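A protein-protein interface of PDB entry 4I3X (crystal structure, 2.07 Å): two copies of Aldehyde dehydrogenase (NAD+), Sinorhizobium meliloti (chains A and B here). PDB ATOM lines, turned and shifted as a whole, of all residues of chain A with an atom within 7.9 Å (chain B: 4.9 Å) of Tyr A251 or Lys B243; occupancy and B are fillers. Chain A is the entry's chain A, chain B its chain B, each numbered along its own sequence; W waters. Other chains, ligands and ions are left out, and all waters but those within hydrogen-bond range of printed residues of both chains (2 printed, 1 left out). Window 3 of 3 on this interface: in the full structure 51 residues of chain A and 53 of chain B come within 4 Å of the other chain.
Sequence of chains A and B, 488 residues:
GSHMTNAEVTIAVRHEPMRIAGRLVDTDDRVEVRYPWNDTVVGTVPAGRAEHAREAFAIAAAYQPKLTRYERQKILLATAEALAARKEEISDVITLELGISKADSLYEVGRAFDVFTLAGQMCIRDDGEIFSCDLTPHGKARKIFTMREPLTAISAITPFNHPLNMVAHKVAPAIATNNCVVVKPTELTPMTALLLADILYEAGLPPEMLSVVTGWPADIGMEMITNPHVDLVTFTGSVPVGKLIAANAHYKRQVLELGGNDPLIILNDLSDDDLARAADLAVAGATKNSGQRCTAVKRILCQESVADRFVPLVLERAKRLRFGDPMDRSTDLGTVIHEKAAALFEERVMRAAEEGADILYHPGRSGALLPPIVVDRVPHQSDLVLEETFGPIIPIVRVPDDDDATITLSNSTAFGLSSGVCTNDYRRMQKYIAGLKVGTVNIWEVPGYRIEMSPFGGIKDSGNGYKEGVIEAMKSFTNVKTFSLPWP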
ATOM      1  N   ILE A 225      -4.081 -20.788   5.114  1.00  0.00           N
ATOM      2  CA  ILE A 225      -3.961 -20.079   6.423  1.00  0.00           C
ATOM      3  C   ILE A 225      -3.984 -21.078   7.560  1.00  0.00           C
ATOM      4  O   ILE A 225      -3.357 -20.853   8.595  1.00  0.00           O
ATOM      5  CB  ILE A 225      -5.183 -19.117   6.575  1.00  0.00           C
ATOM      6  CG1 ILE A 225      -5.097 -18.082   5.465  1.00  0.00           C
ATOM      7  CG2 ILE A 225      -5.256 -18.349   7.910  1.00  0.00           C
ATOM      8  CD1 ILE A 225      -3.648 -17.604   5.303  1.00  0.00           C
ATOM      9  N   PRO A 228      -2.443 -27.795   8.832  1.00  0.00           N
ATOM     10  CA  PRO A 228      -1.735 -28.172  10.061  1.00  0.00           C
ATOM     11  C   PRO A 228      -0.230 -28.204   9.923  1.00  0.00           C
ATOM     12  O   PRO A 228       0.452 -28.001  10.918  1.00  0.00           O
ATOM     13  CB  PRO A 228      -2.331 -29.579  10.435  1.00  0.00           C
ATOM     14  CG  PRO A 228      -3.035 -30.045   9.195  1.00  0.00           C
ATOM     15  CD  PRO A 228      -3.515 -28.764   8.531  1.00  0.00           C
ATOM     16  N   VAL A 230       1.692 -25.969   8.278  1.00  0.00           N
ATOM     17  CA  VAL A 230       2.249 -24.642   8.001  1.00  0.00           C
ATOM     18  C   VAL A 230       2.743 -24.089   9.337  1.00  0.00           C
ATOM     19  O   VAL A 230       1.968 -23.958  10.291  1.00  0.00           O
ATOM     20  CB  VAL A 230       1.172 -23.691   7.379  1.00  0.00           C
ATOM     21  CG1 VAL A 230       1.694 -22.274   7.305  1.00  0.00           C
ATOM     22  CG2 VAL A 230       0.754 -24.169   5.963  1.00  0.00           C
ATOM     23  N   ASP A 231       4.031 -23.826   9.375  1.00  0.00           N
ATOM     24  CA  ASP A 231       4.708 -23.130  10.456  1.00  0.00           C
ATOM     25  C   ASP A 231       4.616 -21.611  10.368  1.00  0.00           C
ATOM     26  O   ASP A 231       4.562 -20.947  11.382  1.00  0.00           O
ATOM     27  CB  ASP A 231       6.200 -23.528  10.460  1.00  0.00           C
ATOM     28  CG  ASP A 231       6.431 -24.926  11.116  1.00  0.00           C
ATOM     29  OD1 ASP A 231       5.431 -25.517  11.595  1.00  0.00           O
ATOM     30  OD2 ASP A 231       7.568 -25.457  11.155  1.00  0.00           O
ATOM     31  N   LEU A 232       4.577 -21.063   9.156  1.00  0.00           N
ATOM     32  CA  LEU A 232       4.650 -19.611   9.007  1.00  0.00           C
ATOM     33  C   LEU A 232       3.792 -19.248   7.791  1.00  0.00           C
ATOM     34  O   LEU A 232       3.939 -19.934   6.746  1.00  0.00           O
ATOM     35  CB  LEU A 232       6.097 -19.155   8.793  1.00  0.00           C
ATOM     36  CG  LEU A 232       6.326 -17.636   8.673  1.00  0.00           C
ATOM     37  CD1 LEU A 232       7.665 -17.235   9.349  1.00  0.00           C
ATOM     38  CD2 LEU A 232       6.399 -17.324   7.193  1.00  0.00           C
ATOM     39  N   ALA A 246      -4.561 -12.576   9.790  1.00  0.00           N
ATOM     40  CA  ALA A 246      -4.142 -12.429  11.189  1.00  0.00           C
ATOM     41  C   ALA A 246      -5.067 -13.153  12.144  1.00  0.00           C
ATOM     42  O   ALA A 246      -4.589 -13.799  13.070  1.00  0.00           O
ATOM     43  CB  ALA A 246      -4.063 -10.998  11.594  1.00  0.00           C
ATOM     44  N   ALA A 247      -6.376 -12.989  11.936  1.00  0.00           N
ATOM     45  CA  ALA A 247      -7.410 -13.501  12.846  1.00  0.00           C
ATOM     46  C   ALA A 247      -7.564 -15.012  12.686  1.00  0.00           C
ATOM     47  O   ALA A 247      -7.977 -15.682  13.656  1.00  0.00           O
ATOM     48  CB  ALA A 247      -8.784 -12.823  12.575  1.00  0.00           C
ATOM     49  N   ASN A 248      -7.279 -15.553  11.472  1.00  0.00           N
ATOM     50  CA  ASN A 248      -7.434 -17.019  11.241  1.00  0.00           C
ATOM     51  C   ASN A 248      -6.216 -17.979  11.318  1.00  0.00           C
ATOM     52  O   ASN A 248      -6.412 -19.217  11.387  1.00  0.00           O
ATOM     53  CB  ASN A 248      -8.277 -17.296  10.007  1.00  0.00           C
ATOM     54  CG  ASN A 248      -9.718 -16.812  10.190  1.00  0.00           C
ATOM     55  OD1 ASN A 248     -10.447 -17.351  11.007  1.00  0.00           O
ATOM     56  ND2 ASN A 248     -10.118 -15.793   9.434  1.00  0.00           N
ATOM     57  N   ALA A 249      -4.994 -17.414  11.363  1.00  0.00           N
ATOM     58  CA  ALA A 249      -3.781 -18.237  11.361  1.00  0.00           C
ATOM     59  C   ALA A 249      -3.353 -18.597  12.786  1.00  0.00           C
ATOM     60  O   ALA A 249      -2.253 -18.275  13.194  1.00  0.00           O
ATOM     61  CB  ALA A 249      -2.638 -17.538  10.613  1.00  0.00           C
ATOM     62  N   HIS A 250      -4.214 -19.294  13.519  1.00  0.00           N
ATOM     63  CA  HIS A 250      -4.036 -19.479  14.952  1.00  0.00           C
ATOM     64  C   HIS A 250      -2.820 -20.276  15.205  1.00  0.00           C
ATOM     65  O   HIS A 250      -2.671 -21.394  14.680  1.00  0.00           O
ATOM     66  CB  HIS A 250      -5.208 -20.248  15.516  1.00  0.00           C
ATOM     67  CG  HIS A 250      -6.536 -19.548  15.340  1.00  0.00           C
ATOM     68  ND1 HIS A 250      -7.714 -20.196  15.444  1.00  0.00           N
ATOM     69  CD2 HIS A 250      -6.841 -18.224  15.014  1.00  0.00           C
ATOM     70  CE1 HIS A 250      -8.731 -19.329  15.245  1.00  0.00           C
ATOM     71  NE2 HIS A 250      -8.196 -18.123  14.954  1.00  0.00           N
ATOM     72  N   TYR A 251      -1.934 -19.711  16.010  1.00  0.00           N
ATOM     73  CA  TYR A 251      -0.720 -20.427  16.460  1.00  0.00           C
ATOM     74  C   TYR A 251       0.283 -20.690  15.298  1.00  0.00           C
ATOM     75  O   TYR A 251       0.927 -21.782  15.187  1.00  0.00           O
ATOM     76  CB  TYR A 251      -1.069 -21.705  17.243  1.00  0.00           C
ATOM     77  CG  TYR A 251       0.114 -22.184  18.109  1.00  0.00           C
ATOM     78  CD1 TYR A 251       0.561 -21.418  19.173  1.00  0.00           C
ATOM     79  CD2 TYR A 251       0.800 -23.369  17.812  1.00  0.00           C
ATOM     80  CE1 TYR A 251       1.633 -21.841  19.969  1.00  0.00           C
ATOM     81  CE2 TYR A 251       1.881 -23.815  18.575  1.00  0.00           C
ATOM     82  CZ  TYR A 251       2.296 -23.060  19.674  1.00  0.00           C
ATOM     83  OH  TYR A 251       3.398 -23.462  20.464  1.00  0.00           O
ATOM     84  N   LYS A 252       0.376 -19.717  14.397  1.00  0.00           N
ATOM     85  CA  LYS A 252       1.341 -19.817  13.331  1.00  0.00           C
ATOM     86  C   LYS A 252       2.075 -18.570  13.393  1.00  0.00           C
ATOM     87  O   LYS A 252       1.531 -17.575  13.861  1.00  0.00           O
ATOM     88  CB  LYS A 252       0.661 -19.963  11.948  1.00  0.00           C
ATOM     89  CG  LYS A 252      -0.006 -21.306  11.829  1.00  0.00           C
ATOM     90  CD  LYS A 252      -0.615 -21.531  10.450  1.00  0.00           C
ATOM     91  CE  LYS A 252      -1.470 -22.796  10.355  1.00  0.00           C
ATOM     92  NZ  LYS A 252      -0.860 -24.090  10.847  1.00  0.00           N
ATOM     93  N   ARG A 253       3.325 -18.566  12.975  1.00  0.00           N
ATOM     94  CA  ARG A 253       3.954 -17.262  12.882  1.00  0.00           C
ATOM     95  C   ARG A 253       3.341 -16.615  11.661  1.00  0.00           C
ATOM     96  O   ARG A 253       2.915 -17.318  10.719  1.00  0.00           O
ATOM     97  CB  ARG A 253       5.463 -17.350  12.739  1.00  0.00           C
ATOM     98  CG  ARG A 253       6.035 -18.469  13.541  1.00  0.00           C
ATOM     99  CD  ARG A 253       7.263 -18.039  14.271  1.00  0.00           C
ATOM    100  NE  ARG A 253       8.496 -18.114  13.501  1.00  0.00           N
ATOM    101  CZ  ARG A 253       9.268 -19.191  13.377  1.00  0.00           C
ATOM    102  NH1 ARG A 253       8.905 -20.400  13.873  1.00  0.00           N
ATOM    103  NH2 ARG A 253      10.406 -19.036  12.700  1.00  0.00           N
ATOM    104  N   GLN A 254       3.303 -15.292  11.692  1.00  0.00           N
ATOM    105  CA  GLN A 254       2.646 -14.504  10.654  1.00  0.00           C
ATOM    106  C   GLN A 254       3.505 -13.354  10.345  1.00  0.00           C
ATOM    107  O   GLN A 254       3.863 -12.585  11.250  1.00  0.00           O
ATOM    108  CB  GLN A 254       1.329 -13.941  11.162  1.00  0.00           C
ATOM    109  CG  GLN A 254       0.219 -14.962  11.313  1.00  0.00           C
ATOM    110  CD  GLN A 254      -0.858 -14.443  12.232  1.00  0.00           C
ATOM    111  OE1 GLN A 254      -1.269 -13.278  12.134  1.00  0.00           O
ATOM    112  NE2 GLN A 254      -1.290 -15.285  13.169  1.00  0.00           N
ATOM    113  N   VAL B 239      -0.098 -24.849  27.622  1.00  0.00           N
ATOM    114  CA  VAL B 239      -0.520 -25.027  26.231  1.00  0.00           C
ATOM    115  C   VAL B 239      -1.968 -24.593  25.980  1.00  0.00           C
ATOM    116  O   VAL B 239      -2.188 -23.799  25.096  1.00  0.00           O
ATOM    117  CB  VAL B 239      -0.260 -26.448  25.712  1.00  0.00           C
ATOM    118  CG1 VAL B 239      -0.718 -26.629  24.260  1.00  0.00           C
ATOM    119  CG2 VAL B 239       1.215 -26.796  25.840  1.00  0.00           C
ATOM    120  N   PRO B 240      -2.958 -25.106  26.748  1.00  0.00           N
ATOM    121  CA  PRO B 240      -4.335 -24.720  26.459  1.00  0.00           C
ATOM    122  C   PRO B 240      -4.557 -23.236  26.578  1.00  0.00           C
ATOM    123  O   PRO B 240      -5.198 -22.631  25.701  1.00  0.00           O
ATOM    124  CB  PRO B 240      -5.149 -25.476  27.530  1.00  0.00           C
ATOM    125  CG  PRO B 240      -4.319 -26.629  27.872  1.00  0.00           C
ATOM    126  CD  PRO B 240      -2.904 -26.100  27.828  1.00  0.00           C
ATOM    127  N   VAL B 241      -4.029 -22.593  27.620  1.00  0.00           N
ATOM    128  CA  VAL B 241      -4.247 -21.143  27.708  1.00  0.00           C
ATOM    129  C   VAL B 241      -3.530 -20.417  26.575  1.00  0.00           C
ATOM    130  O   VAL B 241      -4.086 -19.458  26.001  1.00  0.00           O
ATOM    131  CB  VAL B 241      -3.924 -20.556  29.097  1.00  0.00           C
ATOM    132  CG1 VAL B 241      -4.045 -19.029  29.053  1.00  0.00           C
ATOM    133  CG2 VAL B 241      -4.865 -21.209  30.120  1.00  0.00           C
ATOM    134  N   GLY B 242      -2.342 -20.913  26.201  1.00  0.00           N
ATOM    135  CA  GLY B 242      -1.617 -20.361  25.043  1.00  0.00           C
ATOM    136  C   GLY B 242      -2.413 -20.394  23.722  1.00  0.00           C
ATOM    137  O   GLY B 242      -2.389 -19.440  22.951  1.00  0.00           O
ATOM    138  N   LYS B 243      -3.081 -21.513  23.443  1.00  0.00           N
ATOM    139  CA  LYS B 243      -3.785 -21.673  22.156  1.00  0.00           C
ATOM    140  C   LYS B 243      -5.070 -20.905  22.202  1.00  0.00           C
ATOM    141  O   LYS B 243      -5.523 -20.436  21.178  1.00  0.00           O
ATOM    142  CB  LYS B 243      -4.110 -23.129  21.834  1.00  0.00           C
ATOM    143  CG  LYS B 243      -2.991 -24.069  22.140  1.00  0.00           C
ATOM    144  CD  LYS B 243      -2.098 -24.330  20.980  1.00  0.00           C
ATOM    145  CE  LYS B 243      -1.941 -25.840  20.911  1.00  0.00           C
ATOM    146  NZ  LYS B 243      -0.926 -26.058  19.869  1.00  0.00           N
ATOM    147  N   LEU B 244      -5.617 -20.719  23.396  1.00  0.00           N
ATOM    148  CA  LEU B 244      -6.755 -19.825  23.558  1.00  0.00           C
ATOM    149  C   LEU B 244      -6.356 -18.396  23.159  1.00  0.00           C
ATOM    150  O   LEU B 244      -7.013 -17.807  22.313  1.00  0.00           O
ATOM    151  CB  LEU B 244      -7.369 -19.926  24.984  1.00  0.00           C
ATOM    152  CG  LEU B 244      -8.543 -19.008  25.412  1.00  0.00           C
ATOM    153  CD1 LEU B 244      -9.186 -19.482  26.716  1.00  0.00           C
ATOM    154  CD2 LEU B 244      -8.093 -17.557  25.600  1.00  0.00           C
ATOM    155  N   ILE B 245      -5.273 -17.859  23.754  1.00  0.00           N
ATOM    156  CA  ILE B 245      -4.773 -16.533  23.432  1.00  0.00           C
ATOM    157  C   ILE B 245      -4.444 -16.416  21.924  1.00  0.00           C
ATOM    158  O   ILE B 245      -4.738 -15.393  21.279  1.00  0.00           O
ATOM    159  CB  ILE B 245      -3.556 -16.182  24.335  1.00  0.00           C
ATOM    160  CG1 ILE B 245      -4.047 -16.027  25.772  1.00  0.00           C
ATOM    161  CG2 ILE B 245      -2.823 -14.900  23.909  1.00  0.00           C
ATOM    162  CD1 ILE B 245      -2.929 -15.956  26.770  1.00  0.00           C
ATOM    163  N   ALA B 246      -3.862 -17.466  21.353  1.00  0.00           N
ATOM    164  CA  ALA B 246      -3.529 -17.431  19.931  1.00  0.00           C
ATOM    165  C   ALA B 246      -4.805 -17.342  19.011  1.00  0.00           C
ATOM    166  O   ALA B 246      -4.722 -16.823  17.879  1.00  0.00           O
ATOM    167  CB  ALA B 246      -2.678 -18.662  19.528  1.00  0.00           C
ATOM    168  N   ALA B 247      -5.935 -17.867  19.480  1.00  0.00           N
ATOM    169  CA  ALA B 247      -7.206 -17.751  18.771  1.00  0.00           C
ATOM    170  C   ALA B 247      -7.886 -16.374  18.927  1.00  0.00           C
ATOM    171  O   ALA B 247      -8.960 -16.165  18.326  1.00  0.00           O
ATOM    172  CB  ALA B 247      -8.165 -18.882  19.193  1.00  0.00           C
ATOM    173  N   LEU B 256       4.394 -16.391  22.696  1.00  0.00           N
ATOM    174  CA  LEU B 256       3.731 -17.370  23.535  1.00  0.00           C
ATOM    175  C   LEU B 256       4.766 -18.459  23.879  1.00  0.00           C
ATOM    176  O   LEU B 256       5.332 -19.098  22.970  1.00  0.00           O
ATOM    177  CB  LEU B 256       2.558 -17.970  22.761  1.00  0.00           C
ATOM    178  CG  LEU B 256       1.523 -16.939  22.218  1.00  0.00           C
ATOM    179  CD1 LEU B 256       0.543 -17.621  21.268  1.00  0.00           C
ATOM    180  CD2 LEU B 256       0.733 -16.292  23.347  1.00  0.00           C
ATOM    181  N   LEU B 258       5.103 -21.702  26.080  1.00  0.00           N
ATOM    182  CA  LEU B 258       4.161 -22.613  26.609  1.00  0.00           C
ATOM    183  C   LEU B 258       4.891 -23.843  27.256  1.00  0.00           C
ATOM    184  O   LEU B 258       6.060 -23.765  27.704  1.00  0.00           O
ATOM    185  CB  LEU B 258       3.198 -23.053  25.469  1.00  0.00           C
ATOM    186  CG  LEU B 258       2.059 -22.178  24.970  1.00  0.00           C
ATOM    187  CD1 LEU B 258       2.081 -20.723  25.434  1.00  0.00           C
ATOM    188  CD2 LEU B 258       1.812 -22.299  23.467  1.00  0.00           C
ATOM    189  N   LYS B 460       7.148 -26.512  18.324  1.00  0.00           N
ATOM    190  CA  LYS B 460       6.037 -27.462  18.504  1.00  0.00           C
ATOM    191  C   LYS B 460       5.045 -26.856  19.528  1.00  0.00           C
ATOM    192  O   LYS B 460       4.746 -25.667  19.425  1.00  0.00           O
ATOM    193  CB  LYS B 460       6.565 -28.870  18.876  1.00  0.00           C
ATOM    194  CG  LYS B 460       7.541 -29.457  17.823  1.00  0.00           C
ATOM    195  CD  LYS B 460       8.307 -30.725  18.272  1.00  0.00           C
ATOM    196  CE  LYS B 460       7.428 -31.815  18.914  1.00  0.00           C
ATOM    197  NZ  LYS B 460       8.153 -33.033  19.398  1.00  0.00           N
ATOM    198  N   ASP B 461       4.550 -27.621  20.508  1.00  0.00           N
ATOM    199  CA  ASP B 461       3.621 -27.032  21.435  1.00  0.00           C
ATOM    200  C   ASP B 461       4.280 -26.220  22.501  1.00  0.00           C
ATOM    201  O   ASP B 461       3.590 -25.740  23.356  1.00  0.00           O
ATOM    202  CB  ASP B 461       2.725 -28.071  22.100  1.00  0.00           C
ATOM    203  CG  ASP B 461       1.498 -28.441  21.228  1.00  0.00           C
ATOM    204  OD1 ASP B 461       1.244 -27.770  20.166  1.00  0.00           O
ATOM    205  OD2 ASP B 461       0.789 -29.397  21.621  1.00  0.00           O
ATOM    206  N   SER B 462       5.597 -26.092  22.498  1.00  0.00           N
ATOM    207  CA  SER B 462       6.247 -25.369  23.598  1.00  0.00           C
ATOM    208  C   SER B 462       6.299 -23.870  23.355  1.00  0.00           C
ATOM    209  O   SER B 462       6.640 -23.098  24.269  1.00  0.00           O
ATOM    210  CB  SER B 462       7.665 -25.885  23.847  1.00  0.00           C
ATOM    211  OG  SER B 462       7.627 -27.228  24.320  1.00  0.00           O
ATOM    212  N   GLY B 463       6.042 -23.461  22.120  1.00  0.00           N
ATOM    213  CA  GLY B 463       6.002 -22.047  21.809  1.00  0.00           C
ATOM    214  C   GLY B 463       5.705 -21.767  20.353  1.00  0.00           C
ATOM    215  O   GLY B 463       5.946 -22.609  19.465  1.00  0.00           O
ATOM    216  N   ASN B 464       5.189 -20.570  20.109  1.00  0.00           N
ATOM    217  CA  ASN B 464       4.939 -20.119  18.741  1.00  0.00           C
ATOM    218  C   ASN B 464       6.154 -19.698  17.970  1.00  0.00           C
ATOM    219  O   ASN B 464       5.995 -19.173  16.884  1.00  0.00           O
ATOM    220  CB  ASN B 464       3.771 -19.074  18.634  1.00  0.00           C
ATOM    221  CG  ASN B 464       4.083 -17.683  19.220  1.00  0.00           C
ATOM    222  OD1 ASN B 464       5.009 -17.506  20.009  1.00  0.00           O
ATOM    223  ND2 ASN B 464       3.247 -16.664  18.837  1.00  0.00           N
HETATM  224  O   HOH W   1       1.355 -17.200  16.635  1.00  0.00           O
HETATM  225  O   HOH W   2      -2.499 -16.676  16.463  1.00  0.00           O
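The side-chain hydroxyl (OH) of Tyr A251 sits at hydrogen-bond distance from the backbone carbonyl oxygen (O) of Lys B460, 2.8 Å away.
The side-chain hydroxyl (OH) of Tyr A251 sits close to the backbone carbonyl oxygen (O) of Gly B463, 2.9 Å away.
N of Asn B464 is in hydrogen-bond range of OH of Tyr A251, at 3.4 Å.
His A250 touches Ala B246.
CD2 of His A250 touches CA of Ala B247, at 3.8 Å.
Lys B243 touches Tyr A251 (NZ to CD2, 3.8 Å).
CB of Ala B246 touches N of Tyr A251, at 3.7 Å.
Leu B258 touches Tyr A251.
Tyr A251 touches Asp B461 (OH to C, 3.5 Å).
Tyr A251 touches Ser B462 (OH to N, 3.99 Å).
Arg A253 touches Asn B464 (CD to O, 3.1 Å).
Positions printed for both chains: 246 and 247.
Water W2 bridges O of Ala B246 (2.6 Å) and N of Tyr A251 (3.1 Å).
Water W1 bridges O of Lys A252 (2.8 Å) and ND2 of Asn B464 (3.0 Å).
Printed residues of chain B within 4 Å of Tyr A251: Lys B243, Ala B246, Leu B258, Lys B460, Asp B461, Ser B462, Gly B463 and Asn B464.
Lys B243 touches just one residue of chain A: Tyr A251 (3.8 Å).
No residue of chain A comes within 4 Å of Gly B242.
Gly B463 touches one residue of chain A.
Printed residues of chain B within 4 Å of Arg A253: Asn B464 (3.1 Å).
Of the printed residues of chain A, Ser B462 touches Tyr A251 (3.99 Å).
Printed residues of chain A within 4 Å of Lys B460: Tyr A251.
Of the printed residues of chain A, Asp B461 touches Tyr A251 (3.5 Å).
Val B241 touches none of the printed residues of chain A.
The nearest printed residue of chain B that does not touch Tyr A251 is Leu B256 (4.3 Å).
The nearest printed residue of chain A that does not touch Ala B246 is Ala A247 (5.5 Å).
The backbone carbonyl oxygen (O) of Asp A231 lies within hydrogen-bond range of the backbone NH (N) of Arg A253 (3.1 Å).
The backbone carbonyl oxygen (O) of Ala A247 lies within hydrogen-bond range of a ring nitrogen (NE2) of His A250, at 2.8 Å.
NZ of Lys B243 lies within salt-bridge range of OD1 of Asp B461 (2.8 Å).
N of Leu B256 is in hydrogen-bond range of OD1 of Asn B464 (3.0 Å).
The backbone carbonyl oxygen of Ser B462 sits at hydrogen-bond distance from the backbone NH of Leu B258, 2.8 Å away.
Hydrophobic or aromatic side chains of chain B that line the printed part of chain A: Ala B246, Ala B247 and Leu B258.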
